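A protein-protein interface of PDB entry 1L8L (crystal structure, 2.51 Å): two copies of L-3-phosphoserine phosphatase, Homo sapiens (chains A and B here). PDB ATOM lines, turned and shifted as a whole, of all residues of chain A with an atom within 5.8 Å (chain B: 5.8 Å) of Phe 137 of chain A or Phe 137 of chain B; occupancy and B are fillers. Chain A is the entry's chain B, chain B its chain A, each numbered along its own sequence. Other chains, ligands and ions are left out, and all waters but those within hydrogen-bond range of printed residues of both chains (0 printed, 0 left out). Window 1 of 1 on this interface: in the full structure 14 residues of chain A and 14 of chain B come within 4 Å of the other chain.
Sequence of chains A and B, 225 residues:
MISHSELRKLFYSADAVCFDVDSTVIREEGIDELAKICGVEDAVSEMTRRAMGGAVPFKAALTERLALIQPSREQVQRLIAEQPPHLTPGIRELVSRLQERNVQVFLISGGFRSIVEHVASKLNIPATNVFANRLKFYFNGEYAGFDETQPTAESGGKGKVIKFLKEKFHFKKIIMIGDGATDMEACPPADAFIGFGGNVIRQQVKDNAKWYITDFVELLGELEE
Among the printed residues, pairs that only touch across the chains: Val 76 of chain A with Phe 139 of chain B, Lys 136 of chain A with Phe 137 of chain B, Tyr 138 of chain A with Lys 136 of chain B, Phe 137 of chain A with Lys 136 of chain B, Phe 139 of chain A with Ser 114 of chain B, Ala 144 of chain A with Lys 136 of chain B, Phe 139 of chain A with Phe 137 of chain B, Tyr 138 of chain A with Leu 135 of chain B, Leu 135 of chain A with Phe 139 of chain B, Phe 139 of chain A with Val 76 of chain B, Lys 136 of chain A with Ala 144 of chain B, Leu 135 of chain A with Tyr 138 of chain B, Phe 137 of chain A with Phe 139 of chain B, Ser 114 of chain A with Phe 139 of chain B and Lys 136 of chain A with Tyr 138 of chain B.
O of Phe 139 of chain B is in hydrogen-bond range of NH1 of Arg 73 of chain A.
N of Phe 139 of chain A sits at hydrogen-bond distance from O of Leu 135 of chain B (3.4 Å).
The guanidinium group (NE) of Arg 73 of chain B sits close to the guanidinium group (NH2) of Arg 73 of chain A (3.4 Å).
The backbone carbonyl oxygen (O) of Phe 139 of chain A lies within hydrogen-bond range of the guanidinium group (NH2) of Arg 73 of chain B (3.0 Å).
The backbone NH of Phe 137 of chain B is in hydrogen-bond range of the backbone carbonyl oxygen of Phe 137 of chain A.
The guanidinium group of Arg 73 of chain A is in hydrogen-bond range of the backbone carbonyl oxygen of Tyr 138 of chain B (3.4 Å).
Printed residues of chain B that touch a printed residue of chain A: Arg 73, Val 76, Ser 114, Leu 135, Lys 136, Phe 137, Tyr 138, Phe 139 and Ala 144.
Among the printed residues, 21 pairs touch across the chains.
Val 76 of chain A touches Phe 139 of chain B, and with the chains exchanged Phe 139 of chain A touches Val 76 of chain B.
Leu 135 of chain A touches Phe 139 of chain B, and with the chains exchanged Phe 139 of chain A touches Leu 135 of chain B.
Lys 136 of chain A touches Phe 137 of chain B, and with the chains exchanged Phe 137 of chain A touches Lys 136 of chain B.
Lys 136 of chain A touches Tyr 138 of chain B, and with the chains exchanged Tyr 138 of chain A touches Lys 136 of chain B.
15 positions are printed for both chains.
Phe 137 of chain A touches just these residues of chain B: Lys 136 (3.3 Å), Phe 137 (2.5 Å) and Phe 139 (3.9 Å).
Of chain A, only Lys 136, Phe 137 and Phe 139 come within 4 Å of Phe 137 of chain B.
Of the printed residues of chain B, Val 76 of chain A touches Phe 139 (3.3 Å).
Of the printed residues of chain A, Val 76 of chain B touches Phe 139.
Of the printed residues of chain A, Tyr 138 of chain B touches Arg 73, Leu 135 and Lys 136.
Of the printed residues of chain A, Ala 144 of chain B touches Lys 136 (3.8 Å).
Of the printed residues of chain B, Phe 139 of chain A touches Arg 73 (3.0 Å), Val 76 (3.8 Å), Ser 114 (3.3 Å), Leu 135 (3.4 Å) and Phe 137 (3.4 Å).
Ser 72 of chain B touches none of the printed residues of chain A.
Tyr 143 of chain A touches none of the printed residues of chain B.
The nearest residue of chain B that does not touch Phe 137 of chain A is Tyr 138 of chain B (4.3 Å).
The nearest residue of chain A that does not touch Phe 137 of chain B is Leu 135 of chain A (4.1 Å).
O of Gly 145 of chain B lies within hydrogen-bond range of N of Lys 136 of chain B (3.0 Å).
The backbone carbonyl oxygen (O) of Gly 141 of chain B sits at hydrogen-bond distance from the backbone NH (N) of Arg 73 of chain B, 2.7 Å away.
The backbone carbonyl oxygen (O) of Ala 144 of chain A lies close to the backbone carbonyl oxygen (O) of Lys 136 of chain A.
O of Gly 145 of chain A sits at hydrogen-bond distance from N of Lys 136 of chain A, at 2.7 Å.
N of Ala 144 of chain B is in hydrogen-bond range of O of Lys 136 of chain B.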
ATOM      1  N   PRO A  71     -24.443   0.119 -28.783  1.00  0.00           N
ATOM      2  CA  PRO A  71     -24.461  -0.362 -27.388  1.00  0.00           C
ATOM      3  C   PRO A  71     -25.457   0.275 -26.436  1.00  0.00           C
ATOM      4  O   PRO A  71     -25.580   1.497 -26.378  1.00  0.00           O
ATOM      5  CB  PRO A  71     -23.027  -0.118 -26.936  1.00  0.00           C
ATOM      6  CG  PRO A  71     -22.722   1.186 -27.600  1.00  0.00           C
ATOM      7  CD  PRO A  71     -23.247   0.951 -29.012  1.00  0.00           C
ATOM      8  N   SER A  72     -26.145  -0.558 -25.664  1.00  0.00           N
ATOM      9  CA  SER A  72     -27.152  -0.070 -24.718  1.00  0.00           C
ATOM     10  C   SER A  72     -26.678   0.111 -23.290  1.00  0.00           C
ATOM     11  O   SER A  72     -25.753  -0.550 -22.856  1.00  0.00           O
ATOM     12  CB  SER A  72     -28.324  -1.022 -24.684  1.00  0.00           C
ATOM     13  OG  SER A  72     -27.960  -2.208 -24.023  1.00  0.00           O
ATOM     14  N   ARG A  73     -27.334   0.983 -22.544  1.00  0.00           N
ATOM     15  CA  ARG A  73     -26.930   1.191 -21.169  1.00  0.00           C
ATOM     16  C   ARG A  73     -26.876  -0.139 -20.456  1.00  0.00           C
ATOM     17  O   ARG A  73     -26.196  -0.257 -19.457  1.00  0.00           O
ATOM     18  CB  ARG A  73     -27.915   2.116 -20.451  1.00  0.00           C
ATOM     19  CG  ARG A  73     -27.330   3.462 -20.008  1.00  0.00           C
ATOM     20  CD  ARG A  73     -26.567   3.404 -18.669  1.00  0.00           C
ATOM     21  NE  ARG A  73     -27.409   3.639 -17.496  1.00  0.00           N
ATOM     22  CZ  ARG A  73     -28.034   4.784 -17.206  1.00  0.00           C
ATOM     23  NH1 ARG A  73     -27.936   5.845 -18.000  1.00  0.00           N
ATOM     24  NH2 ARG A  73     -28.757   4.878 -16.089  1.00  0.00           N
ATOM     25  N   GLU A  74     -27.591  -1.137 -20.973  1.00  0.00           N
ATOM     26  CA  GLU A  74     -27.617  -2.466 -20.350  1.00  0.00           C
ATOM     27  C   GLU A  74     -26.354  -3.282 -20.705  1.00  0.00           C
ATOM     28  O   GLU A  74     -25.806  -4.012 -19.872  1.00  0.00           O
ATOM     29  CB  GLU A  74     -28.876  -3.223 -20.790  1.00  0.00           C
ATOM     30  CG  GLU A  74     -30.217  -2.522 -20.464  1.00  0.00           C
ATOM     31  CD  GLU A  74     -30.596  -1.387 -21.444  1.00  0.00           C
ATOM     32  OE1 GLU A  74     -30.613  -1.621 -22.675  1.00  0.00           O
ATOM     33  OE2 GLU A  74     -30.898  -0.260 -20.978  1.00  0.00           O
ATOM     34  N   VAL A  76     -23.397  -1.868 -21.796  1.00  0.00           N
ATOM     35  CA  VAL A  76     -22.126  -1.193 -21.255  1.00  0.00           C
ATOM     36  C   VAL A  76     -22.008  -1.324 -19.776  1.00  0.00           C
ATOM     37  O   VAL A  76     -20.929  -1.437 -19.210  1.00  0.00           O
ATOM     38  CB  VAL A  76     -22.006   0.346 -21.415  1.00  0.00           C
ATOM     39  CG1 VAL A  76     -20.901   0.893 -20.511  1.00  0.00           C
ATOM     40  CG2 VAL A  76     -21.696   0.722 -22.853  1.00  0.00           C
ATOM     41  N   SER A 114     -17.438   5.730 -19.758  1.00  0.00           N
ATOM     42  CA  SER A 114     -18.434   5.018 -19.222  1.00  0.00           C
ATOM     43  C   SER A 114     -17.567   3.884 -18.676  1.00  0.00           C
ATOM     44  O   SER A 114     -17.441   3.691 -17.474  1.00  0.00           O
ATOM     45  CB  SER A 114     -19.335   4.775 -20.478  1.00  0.00           C
ATOM     46  OG  SER A 114     -19.476   6.032 -21.292  1.00  0.00           O
ATOM     47  N   LEU A 135     -20.842   8.591 -23.930  1.00  0.00           N
ATOM     48  CA  LEU A 135     -21.773   7.874 -24.767  1.00  0.00           C
ATOM     49  C   LEU A 135     -23.176   8.238 -24.301  1.00  0.00           C
ATOM     50  O   LEU A 135     -23.537   7.960 -23.153  1.00  0.00           O
ATOM     51  CB  LEU A 135     -21.585   6.373 -24.598  1.00  0.00           C
ATOM     52  CG  LEU A 135     -20.548   5.672 -25.465  1.00  0.00           C
ATOM     53  CD1 LEU A 135     -20.441   4.204 -25.066  1.00  0.00           C
ATOM     54  CD2 LEU A 135     -20.944   5.782 -26.949  1.00  0.00           C
ATOM     55  N   LYS A 136     -23.972   8.843 -25.187  1.00  0.00           N
ATOM     56  CA  LYS A 136     -25.344   9.225 -24.846  1.00  0.00           C
ATOM     57  C   LYS A 136     -26.200   7.973 -24.795  1.00  0.00           C
ATOM     58  O   LYS A 136     -25.847   6.966 -25.397  1.00  0.00           O
ATOM     59  CB  LYS A 136     -25.920  10.197 -25.887  1.00  0.00           C
ATOM     60  CG  LYS A 136     -25.319  11.601 -25.879  1.00  0.00           C
ATOM     61  CD  LYS A 136     -25.166  12.145 -27.292  1.00  0.00           C
ATOM     62  CE  LYS A 136     -24.527  13.504 -27.280  1.00  0.00           C
ATOM     63  NZ  LYS A 136     -23.079  13.295 -27.462  1.00  0.00           N
ATOM     64  N   PHE A 137     -27.323   8.060 -24.082  1.00  0.00           N
ATOM     65  CA  PHE A 137     -28.273   6.949 -23.908  1.00  0.00           C
ATOM     66  C   PHE A 137     -29.743   7.418 -23.750  1.00  0.00           C
ATOM     67  O   PHE A 137     -30.020   8.379 -23.038  1.00  0.00           O
ATOM     68  CB  PHE A 137     -27.888   6.139 -22.661  1.00  0.00           C
ATOM     69  CG  PHE A 137     -26.662   5.275 -22.837  1.00  0.00           C
ATOM     70  CD1 PHE A 137     -26.726   4.103 -23.560  1.00  0.00           C
ATOM     71  CD2 PHE A 137     -25.431   5.650 -22.288  1.00  0.00           C
ATOM     72  CE1 PHE A 137     -25.589   3.331 -23.720  1.00  0.00           C
ATOM     73  CE2 PHE A 137     -24.295   4.868 -22.455  1.00  0.00           C
ATOM     74  CZ  PHE A 137     -24.369   3.720 -23.164  1.00  0.00           C
ATOM     75  N   TYR A 138     -30.691   6.735 -24.381  1.00  0.00           N
ATOM     76  CA  TYR A 138     -32.094   7.117 -24.230  1.00  0.00           C
ATOM     77  C   TYR A 138     -32.584   6.672 -22.847  1.00  0.00           C
ATOM     78  O   TYR A 138     -31.942   5.845 -22.203  1.00  0.00           O
ATOM     79  CB  TYR A 138     -32.959   6.473 -25.334  1.00  0.00           C
ATOM     80  CG  TYR A 138     -32.831   7.160 -26.681  1.00  0.00           C
ATOM     81  CD1 TYR A 138     -32.396   6.468 -27.798  1.00  0.00           C
ATOM     82  CD2 TYR A 138     -33.029   8.525 -26.799  1.00  0.00           C
ATOM     83  CE1 TYR A 138     -32.146   7.123 -29.008  1.00  0.00           C
ATOM     84  CE2 TYR A 138     -32.784   9.196 -27.987  1.00  0.00           C
ATOM     85  CZ  TYR A 138     -32.337   8.499 -29.091  1.00  0.00           C
ATOM     86  OH  TYR A 138     -32.047   9.184 -30.246  1.00  0.00           O
ATOM     87  N   PHE A 139     -33.710   7.227 -22.395  1.00  0.00           N
ATOM     88  CA  PHE A 139     -34.273   6.889 -21.094  1.00  0.00           C
ATOM     89  C   PHE A 139     -34.510   5.399 -21.018  1.00  0.00           C
ATOM     90  O   PHE A 139     -34.350   4.796 -19.965  1.00  0.00           O
ATOM     91  CB  PHE A 139     -35.596   7.628 -20.862  1.00  0.00           C
ATOM     92  CG  PHE A 139     -36.391   7.102 -19.693  1.00  0.00           C
ATOM     93  CD1 PHE A 139     -35.846   7.106 -18.405  1.00  0.00           C
ATOM     94  CD2 PHE A 139     -37.656   6.540 -19.886  1.00  0.00           C
ATOM     95  CE1 PHE A 139     -36.535   6.551 -17.321  1.00  0.00           C
ATOM     96  CE2 PHE A 139     -38.362   5.977 -18.805  1.00  0.00           C
ATOM     97  CZ  PHE A 139     -37.793   5.982 -17.516  1.00  0.00           C
ATOM     98  N   GLY A 141     -32.746   3.365 -22.177  1.00  0.00           N
ATOM     99  CA  GLY A 141     -31.431   2.758 -22.264  1.00  0.00           C
ATOM    100  C   GLY A 141     -31.178   2.108 -23.613  1.00  0.00           C
ATOM    101  O   GLY A 141     -31.315   0.889 -23.741  1.00  0.00           O
ATOM    102  N   GLU A 142     -30.802   2.905 -24.608  1.00  0.00           N
ATOM    103  CA  GLU A 142     -30.535   2.380 -25.933  1.00  0.00           C
ATOM    104  C   GLU A 142     -29.488   3.375 -26.410  1.00  0.00           C
ATOM    105  O   GLU A 142     -29.226   4.348 -25.719  1.00  0.00           O
ATOM    106  CB  GLU A 142     -31.852   2.091 -26.627  1.00  0.00           C
ATOM    107  CG  GLU A 142     -32.906   3.133 -26.307  1.00  0.00           C
ATOM    108  CD  GLU A 142     -34.301   2.744 -26.768  1.00  0.00           C
ATOM    109  OE1 GLU A 142     -35.176   2.556 -25.876  1.00  0.00           O
ATOM    110  OE2 GLU A 142     -34.499   2.634 -28.015  1.00  0.00           O
ATOM    111  N   TYR A 143     -28.882   3.134 -27.572  1.00  0.00           N
ATOM    112  CA  TYR A 143     -27.794   3.991 -28.043  1.00  0.00           C
ATOM    113  C   TYR A 143     -28.499   5.258 -28.479  1.00  0.00           C
ATOM    114  O   TYR A 143     -29.617   5.198 -28.948  1.00  0.00           O
ATOM    115  CB  TYR A 143     -27.061   3.337 -29.220  1.00  0.00           C
ATOM    116  CG  TYR A 143     -25.922   4.173 -29.785  1.00  0.00           C
ATOM    117  CD1 TYR A 143     -25.037   4.822 -28.930  1.00  0.00           C
ATOM    118  CD2 TYR A 143     -25.752   4.341 -31.170  1.00  0.00           C
ATOM    119  CE1 TYR A 143     -24.017   5.626 -29.408  1.00  0.00           C
ATOM    120  CE2 TYR A 143     -24.712   5.155 -31.679  1.00  0.00           C
ATOM    121  CZ  TYR A 143     -23.847   5.791 -30.783  1.00  0.00           C
ATOM    122  OH  TYR A 143     -22.794   6.552 -31.244  1.00  0.00           O
ATOM    123  N   ALA A 144     -27.824   6.395 -28.320  1.00  0.00           N
ATOM    124  CA  ALA A 144     -28.215   7.628 -28.681  1.00  0.00           C
ATOM    125  C   ALA A 144     -26.853   8.016 -28.660  1.00  0.00           C
ATOM    126  O   ALA A 144     -26.114   7.723 -27.729  1.00  0.00           O
ATOM    127  CB  ALA A 144     -28.963   8.245 -27.502  1.00  0.00           C
ATOM    128  N   GLY A 145     -26.378   8.632 -29.737  1.00  0.00           N
ATOM    129  CA  GLY A 145     -24.968   8.943 -29.879  1.00  0.00           C
ATOM    130  C   GLY A 145     -23.933   9.080 -28.771  1.00  0.00           C
ATOM    131  O   GLY A 145     -23.915   8.328 -27.790  1.00  0.00           O
ATOM    132  N   PRO B  71     -32.768  17.529 -16.793  1.00  0.00           N
ATOM    133  CA  PRO B  71     -33.413  16.444 -16.061  1.00  0.00           C
ATOM    134  C   PRO B  71     -32.520  15.215 -16.057  1.00  0.00           C
ATOM    135  O   PRO B  71     -32.304  14.608 -17.096  1.00  0.00           O
ATOM    136  CB  PRO B  71     -34.695  16.235 -16.847  1.00  0.00           C
ATOM    137  CG  PRO B  71     -34.251  16.492 -18.243  1.00  0.00           C
ATOM    138  CD  PRO B  71     -33.419  17.730 -18.098  1.00  0.00           C
ATOM    139  N   SER B  72     -31.979  14.856 -14.901  1.00  0.00           N
ATOM    140  CA  SER B  72     -31.129  13.677 -14.838  1.00  0.00           C
ATOM    141  C   SER B  72     -32.011  12.479 -15.183  1.00  0.00           C
ATOM    142  O   SER B  72     -33.224  12.621 -15.286  1.00  0.00           O
ATOM    143  CB  SER B  72     -30.536  13.539 -13.431  1.00  0.00           C
ATOM    144  OG  SER B  72     -31.199  12.556 -12.650  1.00  0.00           O
ATOM    145  N   ARG B  73     -31.428  11.306 -15.384  1.00  0.00           N
ATOM    146  CA  ARG B  73     -32.264  10.160 -15.691  1.00  0.00           C
ATOM    147  C   ARG B  73     -33.020   9.887 -14.402  1.00  0.00           C
ATOM    148  O   ARG B  73     -34.240   9.796 -14.397  1.00  0.00           O
ATOM    149  CB  ARG B  73     -31.423   8.933 -16.092  1.00  0.00           C
ATOM    150  CG  ARG B  73     -32.222   7.680 -16.578  1.00  0.00           C
ATOM    151  CD  ARG B  73     -31.327   6.416 -16.651  1.00  0.00           C
ATOM    152  NE  ARG B  73     -31.941   5.234 -17.279  1.00  0.00           N
ATOM    153  CZ  ARG B  73     -32.990   4.575 -16.798  1.00  0.00           C
ATOM    154  NH1 ARG B  73     -33.575   4.966 -15.676  1.00  0.00           N
ATOM    155  NH2 ARG B  73     -33.441   3.509 -17.429  1.00  0.00           N
ATOM    156  N   VAL B  76     -36.143  12.054 -13.674  1.00  0.00           N
ATOM    157  CA  VAL B  76     -37.369  11.716 -14.395  1.00  0.00           C
ATOM    158  C   VAL B  76     -37.858  10.368 -13.872  1.00  0.00           C
ATOM    159  O   VAL B  76     -39.016   9.993 -14.068  1.00  0.00           O
ATOM    160  CB  VAL B  76     -37.206  11.646 -15.968  1.00  0.00           C
ATOM    161  CG1 VAL B  76     -36.257  12.714 -16.450  1.00  0.00           C
ATOM    162  CG2 VAL B  76     -36.780  10.260 -16.416  1.00  0.00           C
ATOM    163  N   SER B 114     -40.666   9.231 -21.985  1.00  0.00           N
ATOM    164  CA  SER B 114     -40.465   8.632 -20.667  1.00  0.00           C
ATOM    165  C   SER B 114     -41.773   8.705 -19.907  1.00  0.00           C
ATOM    166  O   SER B 114     -42.281   7.711 -19.398  1.00  0.00           O
ATOM    167  CB  SER B 114     -39.392   9.407 -19.916  1.00  0.00           C
ATOM    168  OG  SER B 114     -38.326   9.686 -20.803  1.00  0.00           O
ATOM    169  N   LEU B 135     -35.973  11.860 -24.537  1.00  0.00           N
ATOM    170  CA  LEU B 135     -34.969  12.462 -23.689  1.00  0.00           C
ATOM    171  C   LEU B 135     -33.711  11.553 -23.740  1.00  0.00           C
ATOM    172  O   LEU B 135     -33.832  10.323 -23.856  1.00  0.00           O
ATOM    173  CB  LEU B 135     -35.569  12.556 -22.287  1.00  0.00           C
ATOM    174  CG  LEU B 135     -35.441  13.865 -21.512  1.00  0.00           C
ATOM    175  CD1 LEU B 135     -35.750  15.064 -22.401  1.00  0.00           C
ATOM    176  CD2 LEU B 135     -36.378  13.809 -20.304  1.00  0.00           C
ATOM    177  N   LYS B 136     -32.518  12.162 -23.690  1.00  0.00           N
ATOM    178  CA  LYS B 136     -31.223  11.442 -23.741  1.00  0.00           C
ATOM    179  C   LYS B 136     -30.354  11.627 -22.480  1.00  0.00           C
ATOM    180  O   LYS B 136     -30.352  12.690 -21.880  1.00  0.00           O
ATOM    181  CB  LYS B 136     -30.399  11.875 -24.984  1.00  0.00           C
ATOM    182  CG  LYS B 136     -30.991  11.409 -26.333  1.00  0.00           C
ATOM    183  CD  LYS B 136     -30.035  11.484 -27.568  1.00  0.00           C
ATOM    184  CE  LYS B 136     -29.926  12.894 -28.168  1.00  0.00           C
ATOM    185  NZ  LYS B 136     -29.282  12.968 -29.517  1.00  0.00           N
ATOM    186  N   PHE B 137     -29.619  10.601 -22.067  1.00  0.00           N
ATOM    187  CA  PHE B 137     -28.778  10.751 -20.883  1.00  0.00           C
ATOM    188  C   PHE B 137     -27.387  10.126 -21.073  1.00  0.00           C
ATOM    189  O   PHE B 137     -27.172   9.310 -21.967  1.00  0.00           O
ATOM    190  CB  PHE B 137     -29.480  10.127 -19.669  1.00  0.00           C
ATOM    191  CG  PHE B 137     -30.950  10.490 -19.546  1.00  0.00           C
ATOM    192  CD1 PHE B 137     -31.346  11.790 -19.204  1.00  0.00           C
ATOM    193  CD2 PHE B 137     -31.934   9.530 -19.781  1.00  0.00           C
ATOM    194  CE1 PHE B 137     -32.691  12.114 -19.104  1.00  0.00           C
ATOM    195  CE2 PHE B 137     -33.269   9.846 -19.683  1.00  0.00           C
ATOM    196  CZ  PHE B 137     -33.654  11.139 -19.346  1.00  0.00           C
ATOM    197  N   TYR B 138     -26.448  10.514 -20.220  1.00  0.00           N
ATOM    198  CA  TYR B 138     -25.098   9.985 -20.278  1.00  0.00           C
ATOM    199  C   TYR B 138     -25.099   8.765 -19.386  1.00  0.00           C
ATOM    200  O   TYR B 138     -26.039   8.549 -18.624  1.00  0.00           O
ATOM    201  CB  TYR B 138     -24.096  11.014 -19.746  1.00  0.00           C
ATOM    202  CG  TYR B 138     -23.871  12.164 -20.692  1.00  0.00           C
ATOM    203  CD1 TYR B 138     -24.318  13.434 -20.403  1.00  0.00           C
ATOM    204  CD2 TYR B 138     -23.284  11.953 -21.934  1.00  0.00           C
ATOM    205  CE1 TYR B 138     -24.190  14.456 -21.336  1.00  0.00           C
ATOM    206  CE2 TYR B 138     -23.153  12.977 -22.868  1.00  0.00           C
ATOM    207  CZ  TYR B 138     -23.611  14.218 -22.564  1.00  0.00           C
ATOM    208  OH  TYR B 138     -23.492  15.216 -23.497  1.00  0.00           O
ATOM    209  N   PHE B 139     -24.059   7.952 -19.481  1.00  0.00           N
ATOM    210  CA  PHE B 139     -23.987   6.789 -18.627  1.00  0.00           C
ATOM    211  C   PHE B 139     -24.288   7.266 -17.197  1.00  0.00           C
ATOM    212  O   PHE B 139     -25.125   6.681 -16.502  1.00  0.00           O
ATOM    213  CB  PHE B 139     -22.591   6.189 -18.714  1.00  0.00           C
ATOM    214  CG  PHE B 139     -22.484   4.807 -18.138  1.00  0.00           C
ATOM    215  CD1 PHE B 139     -22.875   3.703 -18.864  1.00  0.00           C
ATOM    216  CD2 PHE B 139     -21.971   4.612 -16.866  1.00  0.00           C
ATOM    217  CE1 PHE B 139     -22.752   2.438 -18.323  1.00  0.00           C
ATOM    218  CE2 PHE B 139     -21.851   3.344 -16.333  1.00  0.00           C
ATOM    219  CZ  PHE B 139     -22.239   2.265 -17.060  1.00  0.00           C
ATOM    220  N   GLY B 141     -26.001   9.394 -16.178  1.00  0.00           N
ATOM    221  CA  GLY B 141     -27.412   9.714 -16.020  1.00  0.00           C
ATOM    222  C   GLY B 141     -27.708  11.201 -16.099  1.00  0.00           C
ATOM    223  O   GLY B 141     -28.793  11.642 -15.723  1.00  0.00           O
ATOM    224  N   GLU B 142     -26.739  11.967 -16.585  1.00  0.00           N
ATOM    225  CA  GLU B 142     -26.896  13.403 -16.707  1.00  0.00           C
ATOM    226  C   GLU B 142     -27.616  13.766 -18.004  1.00  0.00           C
ATOM    227  O   GLU B 142     -27.648  12.979 -18.951  1.00  0.00           O
ATOM    228  CB  GLU B 142     -25.530  14.093 -16.659  1.00  0.00           C
ATOM    229  CG  GLU B 142     -24.710  13.846 -15.380  1.00  0.00           C
ATOM    230  CD  GLU B 142     -23.228  14.232 -15.542  1.00  0.00           C
ATOM    231  OE1 GLU B 142     -22.939  15.432 -15.770  1.00  0.00           O
ATOM    232  OE2 GLU B 142     -22.362  13.324 -15.449  1.00  0.00           O
ATOM    233  N   TYR B 143     -28.198  14.962 -18.043  1.00  0.00           N
ATOM    234  CA  TYR B 143     -28.917  15.380 -19.225  1.00  0.00           C
ATOM    235  C   TYR B 143     -28.054  15.533 -20.448  1.00  0.00           C
ATOM    236  O   TYR B 143     -27.175  16.398 -20.498  1.00  0.00           O
ATOM    237  CB  TYR B 143     -29.554  16.759 -19.042  1.00  0.00           C
ATOM    238  CG  TYR B 143     -30.307  17.235 -20.265  1.00  0.00           C
ATOM    239  CD1 TYR B 143     -31.407  16.525 -20.750  1.00  0.00           C
ATOM    240  CD2 TYR B 143     -29.881  18.369 -20.968  1.00  0.00           C
ATOM    241  CE1 TYR B 143     -32.064  16.926 -21.914  1.00  0.00           C
ATOM    242  CE2 TYR B 143     -30.522  18.785 -22.133  1.00  0.00           C
ATOM    243  CZ  TYR B 143     -31.619  18.058 -22.609  1.00  0.00           C
ATOM    244  OH  TYR B 143     -32.244  18.460 -23.779  1.00  0.00           O
ATOM    245  N   ALA B 144     -28.308  14.673 -21.427  1.00  0.00           N
ATOM    246  CA  ALA B 144     -27.577  14.683 -22.682  1.00  0.00           C
ATOM    247  C   ALA B 144     -28.294  15.393 -23.826  1.00  0.00           C
ATOM    248  O   ALA B 144     -27.669  15.756 -24.817  1.00  0.00           O
ATOM    249  CB  ALA B 144     -27.311  13.232 -23.042  1.00  0.00           C
ATOM    250  N   GLY B 145     -29.168  15.812 -24.334  1.00  0.00           N
ATOM    251  CA  GLY B 145     -30.443  16.457 -24.784  1.00  0.00           C
ATOM    252  C   GLY B 145     -31.668  15.509 -25.044  1.00  0.00           C
ATOM    253  O   GLY B 145     -32.367  15.091 -24.130  1.00  0.00           O
